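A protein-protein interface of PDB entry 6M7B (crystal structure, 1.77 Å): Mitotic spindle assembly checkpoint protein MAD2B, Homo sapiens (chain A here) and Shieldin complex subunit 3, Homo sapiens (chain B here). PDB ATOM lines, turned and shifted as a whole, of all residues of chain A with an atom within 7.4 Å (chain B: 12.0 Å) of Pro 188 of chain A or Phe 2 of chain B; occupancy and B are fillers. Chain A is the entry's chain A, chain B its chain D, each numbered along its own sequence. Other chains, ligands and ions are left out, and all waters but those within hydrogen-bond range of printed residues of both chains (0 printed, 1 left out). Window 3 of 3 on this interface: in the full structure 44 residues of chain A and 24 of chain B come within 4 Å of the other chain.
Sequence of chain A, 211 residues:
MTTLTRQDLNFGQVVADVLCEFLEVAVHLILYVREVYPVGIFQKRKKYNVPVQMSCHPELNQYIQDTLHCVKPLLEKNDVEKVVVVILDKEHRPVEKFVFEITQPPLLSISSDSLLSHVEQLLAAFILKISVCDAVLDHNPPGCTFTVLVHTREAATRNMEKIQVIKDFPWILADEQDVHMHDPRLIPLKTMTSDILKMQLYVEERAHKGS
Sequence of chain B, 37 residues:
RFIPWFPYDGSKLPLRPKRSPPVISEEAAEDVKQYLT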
ATOM      1  N   GLU A 101     -33.055 -25.427  16.461  1.00  0.00           N
ATOM      2  CA  GLU A 101     -34.268 -25.195  15.693  1.00  0.00           C
ATOM      3  C   GLU A 101     -34.156 -25.926  14.363  1.00  0.00           C
ATOM      4  O   GLU A 101     -33.086 -25.963  13.750  1.00  0.00           O
ATOM      5  CB  GLU A 101     -34.494 -23.698  15.456  1.00  0.00           C
ATOM      6  CG  GLU A 101     -34.509 -22.830  16.700  1.00  0.00           C
ATOM      7  CD  GLU A 101     -35.000 -21.417  16.389  1.00  0.00           C
ATOM      8  OE1 GLU A 101     -35.903 -20.919  17.087  1.00  0.00           O
ATOM      9  OE2 GLU A 101     -34.486 -20.806  15.421  1.00  0.00           O
ATOM     10  N   LYS A 129     -18.121 -26.167  16.271  1.00  0.00           N
ATOM     11  CA  LYS A 129     -18.477 -24.935  16.969  1.00  0.00           C
ATOM     12  C   LYS A 129     -18.805 -25.209  18.429  1.00  0.00           C
ATOM     13  O   LYS A 129     -18.348 -24.486  19.318  1.00  0.00           O
ATOM     14  CB  LYS A 129     -19.663 -24.258  16.281  1.00  0.00           C
ATOM     15  CG  LYS A 129     -19.938 -22.813  16.739  1.00  0.00           C
ATOM     16  CD  LYS A 129     -18.653 -21.968  16.872  1.00  0.00           C
ATOM     17  CE  LYS A 129     -18.982 -20.473  17.032  1.00  0.00           C
ATOM     18  NZ  LYS A 129     -19.722 -19.957  15.817  1.00  0.00           N
ATOM     19  N   VAL A 136     -17.250 -18.164  23.202  1.00  0.00           N
ATOM     20  CA  VAL A 136     -18.228 -17.157  22.802  1.00  0.00           C
ATOM     21  C   VAL A 136     -19.370 -17.020  23.800  1.00  0.00           C
ATOM     22  O   VAL A 136     -20.227 -16.150  23.624  1.00  0.00           O
ATOM     23  CB  VAL A 136     -18.784 -17.436  21.388  1.00  0.00           C
ATOM     24  CG1 VAL A 136     -17.640 -17.586  20.395  1.00  0.00           C
ATOM     25  CG2 VAL A 136     -19.675 -18.678  21.391  1.00  0.00           C
ATOM     26  N   LEU A 137     -19.400 -17.839  24.841  1.00  0.00           N
ATOM     27  CA  LEU A 137     -20.445 -17.798  25.857  1.00  0.00           C
ATOM     28  C   LEU A 137     -19.906 -17.162  27.134  1.00  0.00           C
ATOM     29  O   LEU A 137     -18.691 -17.060  27.341  1.00  0.00           O
ATOM     30  CB  LEU A 137     -20.964 -19.215  26.146  1.00  0.00           C
ATOM     31  CG  LEU A 137     -21.539 -19.970  24.937  1.00  0.00           C
ATOM     32  CD1 LEU A 137     -21.952 -21.378  25.308  1.00  0.00           C
ATOM     33  CD2 LEU A 137     -22.709 -19.218  24.314  1.00  0.00           C
ATOM     34  N   ARG A 185     -29.935 -13.489  26.882  1.00  0.00           N
ATOM     35  CA  ARG A 185     -29.134 -13.141  25.716  1.00  0.00           C
ATOM     36  C   ARG A 185     -29.040 -14.349  24.794  1.00  0.00           C
ATOM     37  O   ARG A 185     -28.736 -15.465  25.232  1.00  0.00           O
ATOM     38  CB  ARG A 185     -27.729 -12.685  26.109  1.00  0.00           C
ATOM     39  CG  ARG A 185     -27.653 -11.707  27.260  1.00  0.00           C
ATOM     40  CD  ARG A 185     -26.191 -11.479  27.605  1.00  0.00           C
ATOM     41  NE  ARG A 185     -25.353 -11.734  26.438  1.00  0.00           N
ATOM     42  CZ  ARG A 185     -24.037 -11.888  26.477  1.00  0.00           C
ATOM     43  NH1 ARG A 185     -23.356 -12.115  25.360  1.00  0.00           N
ATOM     44  NH2 ARG A 185     -23.405 -11.823  27.635  1.00  0.00           N
ATOM     45  N   LEU A 186     -29.306 -14.124  23.518  1.00  0.00           N
ATOM     46  CA  LEU A 186     -29.307 -15.174  22.512  1.00  0.00           C
ATOM     47  C   LEU A 186     -27.979 -15.125  21.767  1.00  0.00           C
ATOM     48  O   LEU A 186     -27.640 -14.098  21.167  1.00  0.00           O
ATOM     49  CB  LEU A 186     -30.485 -14.990  21.550  1.00  0.00           C
ATOM     50  CG  LEU A 186     -31.885 -14.937  22.172  1.00  0.00           C
ATOM     51  CD1 LEU A 186     -32.957 -15.085  21.105  1.00  0.00           C
ATOM     52  CD2 LEU A 186     -32.052 -16.018  23.223  1.00  0.00           C
ATOM     53  N   ILE A 187     -27.233 -16.227  21.810  1.00  0.00           N
ATOM     54  CA  ILE A 187     -25.922 -16.296  21.166  1.00  0.00           C
ATOM     55  C   ILE A 187     -25.967 -17.297  20.017  1.00  0.00           C
ATOM     56  O   ILE A 187     -25.946 -18.508  20.262  1.00  0.00           O
ATOM     57  CB  ILE A 187     -24.819 -16.675  22.176  1.00  0.00           C
ATOM     58  CG1 ILE A 187     -24.911 -15.811  23.437  1.00  0.00           C
ATOM     59  CG2 ILE A 187     -23.427 -16.545  21.534  1.00  0.00           C
ATOM     60  CD1 ILE A 187     -24.645 -14.343  23.207  1.00  0.00           C
ATOM     61  N   PRO A 188     -26.029 -16.860  18.758  1.00  0.00           N
ATOM     62  CA  PRO A 188     -26.031 -17.827  17.649  1.00  0.00           C
ATOM     63  C   PRO A 188     -24.695 -18.543  17.537  1.00  0.00           C
ATOM     64  O   PRO A 188     -23.627 -17.937  17.656  1.00  0.00           O
ATOM     65  CB  PRO A 188     -26.308 -16.959  16.411  1.00  0.00           C
ATOM     66  CG  PRO A 188     -25.822 -15.600  16.799  1.00  0.00           C
ATOM     67  CD  PRO A 188     -26.152 -15.476  18.277  1.00  0.00           C
ATOM     68  N   LEU A 189     -24.759 -19.857  17.338  1.00  0.00           N
ATOM     69  CA  LEU A 189     -23.561 -20.666  17.156  1.00  0.00           C
ATOM     70  C   LEU A 189     -23.377 -21.106  15.711  1.00  0.00           C
ATOM     71  O   LEU A 189     -22.287 -20.971  15.157  1.00  0.00           O
ATOM     72  CB  LEU A 189     -23.617 -21.891  18.082  1.00  0.00           C
ATOM     73  CG  LEU A 189     -23.539 -21.610  19.600  1.00  0.00           C
ATOM     74  CD1 LEU A 189     -23.433 -22.916  20.372  1.00  0.00           C
ATOM     75  CD2 LEU A 189     -22.372 -20.699  19.956  1.00  0.00           C
ATOM     76  N   LYS A 190     -24.422 -21.615  15.064  1.00  0.00           N
ATOM     77  CA  LYS A 190     -24.270 -22.079  13.685  1.00  0.00           C
ATOM     78  C   LYS A 190     -25.641 -22.245  13.039  1.00  0.00           C
ATOM     79  O   LYS A 190     -26.625 -22.556  13.715  1.00  0.00           O
ATOM     80  CB  LYS A 190     -23.489 -23.402  13.619  1.00  0.00           C
ATOM     81  CG  LYS A 190     -22.985 -23.725  12.195  1.00  0.00           C
ATOM     82  CD  LYS A 190     -21.727 -22.885  11.888  1.00  0.00           C
ATOM     83  CE  LYS A 190     -21.198 -23.080  10.464  1.00  0.00           C
ATOM     84  NZ  LYS A 190     -22.018 -22.371   9.416  1.00  0.00           N
ATOM     85  N   THR A 191     -25.695 -22.006  11.729  1.00  0.00           N
ATOM     86  CA  THR A 191     -26.892 -22.193  10.919  1.00  0.00           C
ATOM     87  C   THR A 191     -26.499 -22.952   9.661  1.00  0.00           C
ATOM     88  O   THR A 191     -25.369 -22.838   9.176  1.00  0.00           O
ATOM     89  CB  THR A 191     -27.555 -20.848  10.543  1.00  0.00           C
ATOM     90  OG1 THR A 191     -27.906 -20.142  11.736  1.00  0.00           O
ATOM     91  CG2 THR A 191     -28.836 -21.061   9.717  1.00  0.00           C
ATOM     92  N   GLN A 200     -30.761 -24.354  12.917  1.00  0.00           N
ATOM     93  CA  GLN A 200     -29.872 -23.381  13.521  1.00  0.00           C
ATOM     94  C   GLN A 200     -29.780 -23.639  15.016  1.00  0.00           C
ATOM     95  O   GLN A 200     -30.729 -24.101  15.656  1.00  0.00           O
ATOM     96  CB  GLN A 200     -30.277 -21.936  13.216  1.00  0.00           C
ATOM     97  CG  GLN A 200     -31.453 -21.332  13.927  1.00  0.00           C
ATOM     98  CD  GLN A 200     -31.692 -19.876  13.468  1.00  0.00           C
ATOM     99  OE1 GLN A 200     -30.895 -19.305  12.717  1.00  0.00           O
ATOM    100  NE2 GLN A 200     -32.793 -19.287  13.911  1.00  0.00           N
ATOM    101  N   LEU A 201     -28.591 -23.381  15.542  1.00  0.00           N
ATOM    102  CA  LEU A 201     -28.268 -23.609  16.942  1.00  0.00           C
ATOM    103  C   LEU A 201     -27.902 -22.269  17.548  1.00  0.00           C
ATOM    104  O   LEU A 201     -27.038 -21.560  17.016  1.00  0.00           O
ATOM    105  CB  LEU A 201     -27.104 -24.598  17.084  1.00  0.00           C
ATOM    106  CG  LEU A 201     -26.495 -24.704  18.484  1.00  0.00           C
ATOM    107  CD1 LEU A 201     -27.518 -25.263  19.468  1.00  0.00           C
ATOM    108  CD2 LEU A 201     -25.243 -25.576  18.453  1.00  0.00           C
ATOM    109  N   TYR A 202     -28.585 -21.904  18.627  1.00  0.00           N
ATOM    110  CA  TYR A 202     -28.178 -20.753  19.412  1.00  0.00           C
ATOM    111  C   TYR A 202     -28.340 -21.097  20.884  1.00  0.00           C
ATOM    112  O   TYR A 202     -28.951 -22.109  21.248  1.00  0.00           O
ATOM    113  CB  TYR A 202     -28.979 -19.504  19.055  1.00  0.00           C
ATOM    114  CG  TYR A 202     -30.456 -19.620  19.354  1.00  0.00           C
ATOM    115  CD1 TYR A 202     -31.332 -20.144  18.408  1.00  0.00           C
ATOM    116  CD2 TYR A 202     -30.979 -19.193  20.571  1.00  0.00           C
ATOM    117  CE1 TYR A 202     -32.684 -20.247  18.668  1.00  0.00           C
ATOM    118  CE2 TYR A 202     -32.352 -19.297  20.837  1.00  0.00           C
ATOM    119  CZ  TYR A 202     -33.189 -19.824  19.873  1.00  0.00           C
ATOM    120  OH  TYR A 202     -34.546 -19.928  20.112  1.00  0.00           O
ATOM    121  N   VAL A 203     -27.737 -20.272  21.726  1.00  0.00           N
ATOM    122  CA  VAL A 203     -27.712 -20.501  23.168  1.00  0.00           C
ATOM    123  C   VAL A 203     -28.516 -19.397  23.831  1.00  0.00           C
ATOM    124  O   VAL A 203     -28.362 -18.220  23.482  1.00  0.00           O
ATOM    125  CB  VAL A 203     -26.272 -20.526  23.712  1.00  0.00           C
ATOM    126  CG1 VAL A 203     -26.296 -20.648  25.252  1.00  0.00           C
ATOM    127  CG2 VAL A 203     -25.499 -21.672  23.102  1.00  0.00           C
ATOM    128  N   PHE B   2     -30.233 -10.829  16.741  1.00  0.00           N
ATOM    129  CA  PHE B   2     -30.535 -12.182  16.274  1.00  0.00           C
ATOM    130  C   PHE B   2     -31.969 -12.576  16.605  1.00  0.00           C
ATOM    131  O   PHE B   2     -32.424 -12.408  17.740  1.00  0.00           O
ATOM    132  CB  PHE B   2     -29.569 -13.200  16.887  1.00  0.00           C
ATOM    133  CG  PHE B   2     -29.913 -14.627  16.560  1.00  0.00           C
ATOM    134  CD1 PHE B   2     -29.573 -15.171  15.331  1.00  0.00           C
ATOM    135  CD2 PHE B   2     -30.590 -15.419  17.472  1.00  0.00           C
ATOM    136  CE1 PHE B   2     -29.901 -16.478  15.024  1.00  0.00           C
ATOM    137  CE2 PHE B   2     -30.919 -16.725  17.170  1.00  0.00           C
ATOM    138  CZ  PHE B   2     -30.578 -17.254  15.944  1.00  0.00           C
ATOM    139  N   ILE B   3     -32.671 -13.128  15.620  1.00  0.00           N
ATOM    140  CA  ILE B   3     -34.063 -13.526  15.770  1.00  0.00           C
ATOM    141  C   ILE B   3     -34.180 -15.031  15.545  1.00  0.00           C
ATOM    142  O   ILE B   3     -33.818 -15.533  14.476  1.00  0.00           O
ATOM    143  CB  ILE B   3     -34.996 -12.750  14.822  1.00  0.00           C
ATOM    144  CG1 ILE B   3     -34.539 -12.866  13.361  1.00  0.00           C
ATOM    145  CG2 ILE B   3     -35.065 -11.286  15.241  1.00  0.00           C
ATOM    146  CD1 ILE B   3     -35.426 -13.769  12.502  1.00  0.00           C
ATOM    147  N   PRO B   4     -34.649 -15.794  16.521  1.00  0.00           N
ATOM    148  CA  PRO B   4     -34.891 -17.220  16.290  1.00  0.00           C
ATOM    149  C   PRO B   4     -36.109 -17.448  15.406  1.00  0.00           C
ATOM    150  O   PRO B   4     -36.993 -16.596  15.278  1.00  0.00           O
ATOM    151  CB  PRO B   4     -35.126 -17.770  17.698  1.00  0.00           C
ATOM    152  CG  PRO B   4     -35.554 -16.580  18.501  1.00  0.00           C
ATOM    153  CD  PRO B   4     -34.805 -15.423  17.937  1.00  0.00           C
ATOM    154  N   TRP B   5     -36.143 -18.637  14.803  1.00  0.00           N
ATOM    155  CA  TRP B   5     -37.310 -19.069  14.039  1.00  0.00           C
ATOM    156  C   TRP B   5     -38.520 -19.306  14.936  1.00  0.00           C
ATOM    157  O   TRP B   5     -39.656 -19.057  14.522  1.00  0.00           O
ATOM    158  CB  TRP B   5     -36.990 -20.353  13.257  1.00  0.00           C
ATOM    159  CG  TRP B   5     -35.830 -20.240  12.313  1.00  0.00           C
ATOM    160  CD1 TRP B   5     -35.296 -19.092  11.818  1.00  0.00           C
ATOM    161  CD2 TRP B   5     -35.067 -21.322  11.735  1.00  0.00           C
ATOM    162  NE1 TRP B   5     -34.242 -19.383  10.975  1.00  0.00           N
ATOM    163  CE2 TRP B   5     -34.082 -20.743  10.910  1.00  0.00           C
ATOM    164  CE3 TRP B   5     -35.119 -22.717  11.845  1.00  0.00           C
ATOM    165  CZ2 TRP B   5     -33.157 -21.509  10.196  1.00  0.00           C
ATOM    166  CZ3 TRP B   5     -34.195 -23.480  11.132  1.00  0.00           C
ATOM    167  CH2 TRP B   5     -33.228 -22.871  10.325  1.00  0.00           C
ATOM    168  N   PHE B   6     -38.311 -19.792  16.158  1.00  0.00           N
ATOM    169  CA  PHE B   6     -39.398 -20.188  17.051  1.00  0.00           C
ATOM    170  C   PHE B   6     -39.202 -19.505  18.398  1.00  0.00           C
ATOM    171  O   PHE B   6     -38.703 -20.116  19.353  1.00  0.00           O
ATOM    172  CB  PHE B   6     -39.463 -21.709  17.182  1.00  0.00           C
ATOM    173  CG  PHE B   6     -39.498 -22.422  15.859  1.00  0.00           C
ATOM    174  CD1 PHE B   6     -40.602 -22.307  15.025  1.00  0.00           C
ATOM    175  CD2 PHE B   6     -38.427 -23.191  15.439  1.00  0.00           C
ATOM    176  CE1 PHE B   6     -40.640 -22.954  13.802  1.00  0.00           C
ATOM    177  CE2 PHE B   6     -38.455 -23.846  14.208  1.00  0.00           C
ATOM    178  CZ  PHE B   6     -39.565 -23.724  13.392  1.00  0.00           C
ATOM    179  N   PRO B   7     -39.595 -18.237  18.512  1.00  0.00           N
ATOM    180  CA  PRO B   7     -39.424 -17.518  19.780  1.00  0.00           C
ATOM    181  C   PRO B   7     -40.242 -18.148  20.897  1.00  0.00           C
ATOM    182  O   PRO B   7     -41.182 -18.909  20.660  1.00  0.00           O
ATOM    183  CB  PRO B   7     -39.918 -16.105  19.456  1.00  0.00           C
ATOM    184  CG  PRO B   7     -40.843 -16.290  18.293  1.00  0.00           C
ATOM    185  CD  PRO B   7     -40.231 -17.401  17.483  1.00  0.00           C
ATOM    186  N   TYR B   8     -39.858 -17.819  22.133  1.00  0.00           N
ATOM    187  CA  TYR B   8     -40.534 -18.356  23.308  1.00  0.00           C
ATOM    188  C   TYR B   8     -42.034 -18.122  23.204  1.00  0.00           C
ATOM    189  O   TYR B   8     -42.480 -17.026  22.859  1.00  0.00           O
ATOM    190  CB  TYR B   8     -39.987 -17.701  24.580  1.00  0.00           C
ATOM    191  CG  TYR B   8     -40.730 -18.081  25.844  1.00  0.00           C
ATOM    192  CD1 TYR B   8     -40.491 -19.303  26.468  1.00  0.00           C
ATOM    193  CD2 TYR B   8     -41.673 -17.226  26.413  1.00  0.00           C
ATOM    194  CE1 TYR B   8     -41.165 -19.664  27.624  1.00  0.00           C
ATOM    195  CE2 TYR B   8     -42.357 -17.579  27.569  1.00  0.00           C
ATOM    196  CZ  TYR B   8     -42.094 -18.805  28.169  1.00  0.00           C
ATOM    197  OH  TYR B   8     -42.756 -19.179  29.319  1.00  0.00           O
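The side-chain carboxylate of Glu 101 of chain A lies within hydrogen-bond range of the side-chain amide nitrogen of Gln 200 of chain A.
The side-chain carboxylate (OE1) of Glu 101 of chain A lies within hydrogen-bond range of the side-chain hydroxyl (OH) of Tyr 202 of chain A (3.5 Å).
The side-chain amide oxygen (OE1) of Gln 200 of chain A sits at hydrogen-bond distance from the side-chain hydroxyl (OG1) of Thr 191 of chain A, 3.3 Å away.
Among the printed residues, merely in contact across the chains: Tyr 202 of chain A with Pro 4 of chain B (3.3 Å), Glu 101 of chain A with Pro 4 of chain B (3.3 Å), Gln 200 of chain A with Phe 2 of chain B (3.6 Å), Tyr 202 of chain A with Phe 2 of chain B (3.7 Å), Leu 186 of chain A with Pro 4 of chain B (3.7 Å), Gln 200 of chain A with Pro 4 of chain B (3.8 Å), Pro 188 of chain A with Phe 2 of chain B (3.9 Å) and Gln 200 of chain A with Ile 3 of chain B (3.9 Å).
Of the 15 printed residues of chain A, 5 touch a printed residue of chain B.
Printed residues of chain A that touch a printed residue of chain B: Glu 101, Leu 186, Pro 188, Gln 200 and Tyr 202.
Hydrophobic or aromatic side chains of chain A within 4 Å of the printed part of chain B: Leu 186, Pro 188 and Tyr 202.
Of the 7 printed residues of chain B, 5 touch a printed residue of chain A.
Printed residues of chain B that touch a printed residue of chain A: Phe 2, Ile 3, Pro 4, Trp 5 and Phe 6.
Hydrophobic or aromatic side chains of chain B that line the printed part of chain A: Phe 2, Pro 4, Trp 5 and Phe 6.
Among the printed residues, 11 pairs touch across the chains.
Among the printed residues, no Asp or Glu carboxylate lies within 4 Å of a Lys or Arg side-chain nitrogen of the other chain.
Leu 186 of chain A touches just one residue of chain B: Pro 4.
Of chain B, only Phe 2 (3.9 Å) comes within 4 Å of Pro 188 of chain A.
Gln 200 of chain A touches four residues of chain B.
No residue of chain B comes within 4 Å of Leu 201 of chain A.
Tyr 202 of chain A touches just these residues of chain B: Phe 2 (3.7 Å) and Pro 4 (3.3 Å).
No residue of chain B comes within 4 Å of Val 203 of chain A.
Phe 2 of chain B touches just these residues of chain A: Pro 188 (3.9 Å), Gln 200 (3.6 Å) and Tyr 202 (3.7 Å).
Of the printed residues of chain A, Pro 4 of chain B touches Glu 101, Leu 186, Gln 200 and Tyr 202.
Of the printed residues of chain A, Phe 6 of chain B touches Glu 101.
Tyr 8 of chain B touches none of the printed residues of chain A.
The nearest residue of chain B that does not touch Pro 188 of chain A is Ile 3 of chain B (7.4 Å).
The nearest printed residue of chain A that does not touch Trp 5 of chain B is Thr 191 of chain A (4.4 Å).
The side-chain carboxylate of Glu 101 of chain A lies within hydrogen-bond range of the backbone NH of Trp 5 of chain B (2.8 Å).
OE1 of Glu 101 of chain A sits at hydrogen-bond distance from N of Phe 6 of chain B (2.8 Å).
NE2 of Gln 200 of chain A sits close to NE1 of Trp 5 of chain B, 3.3 Å away.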
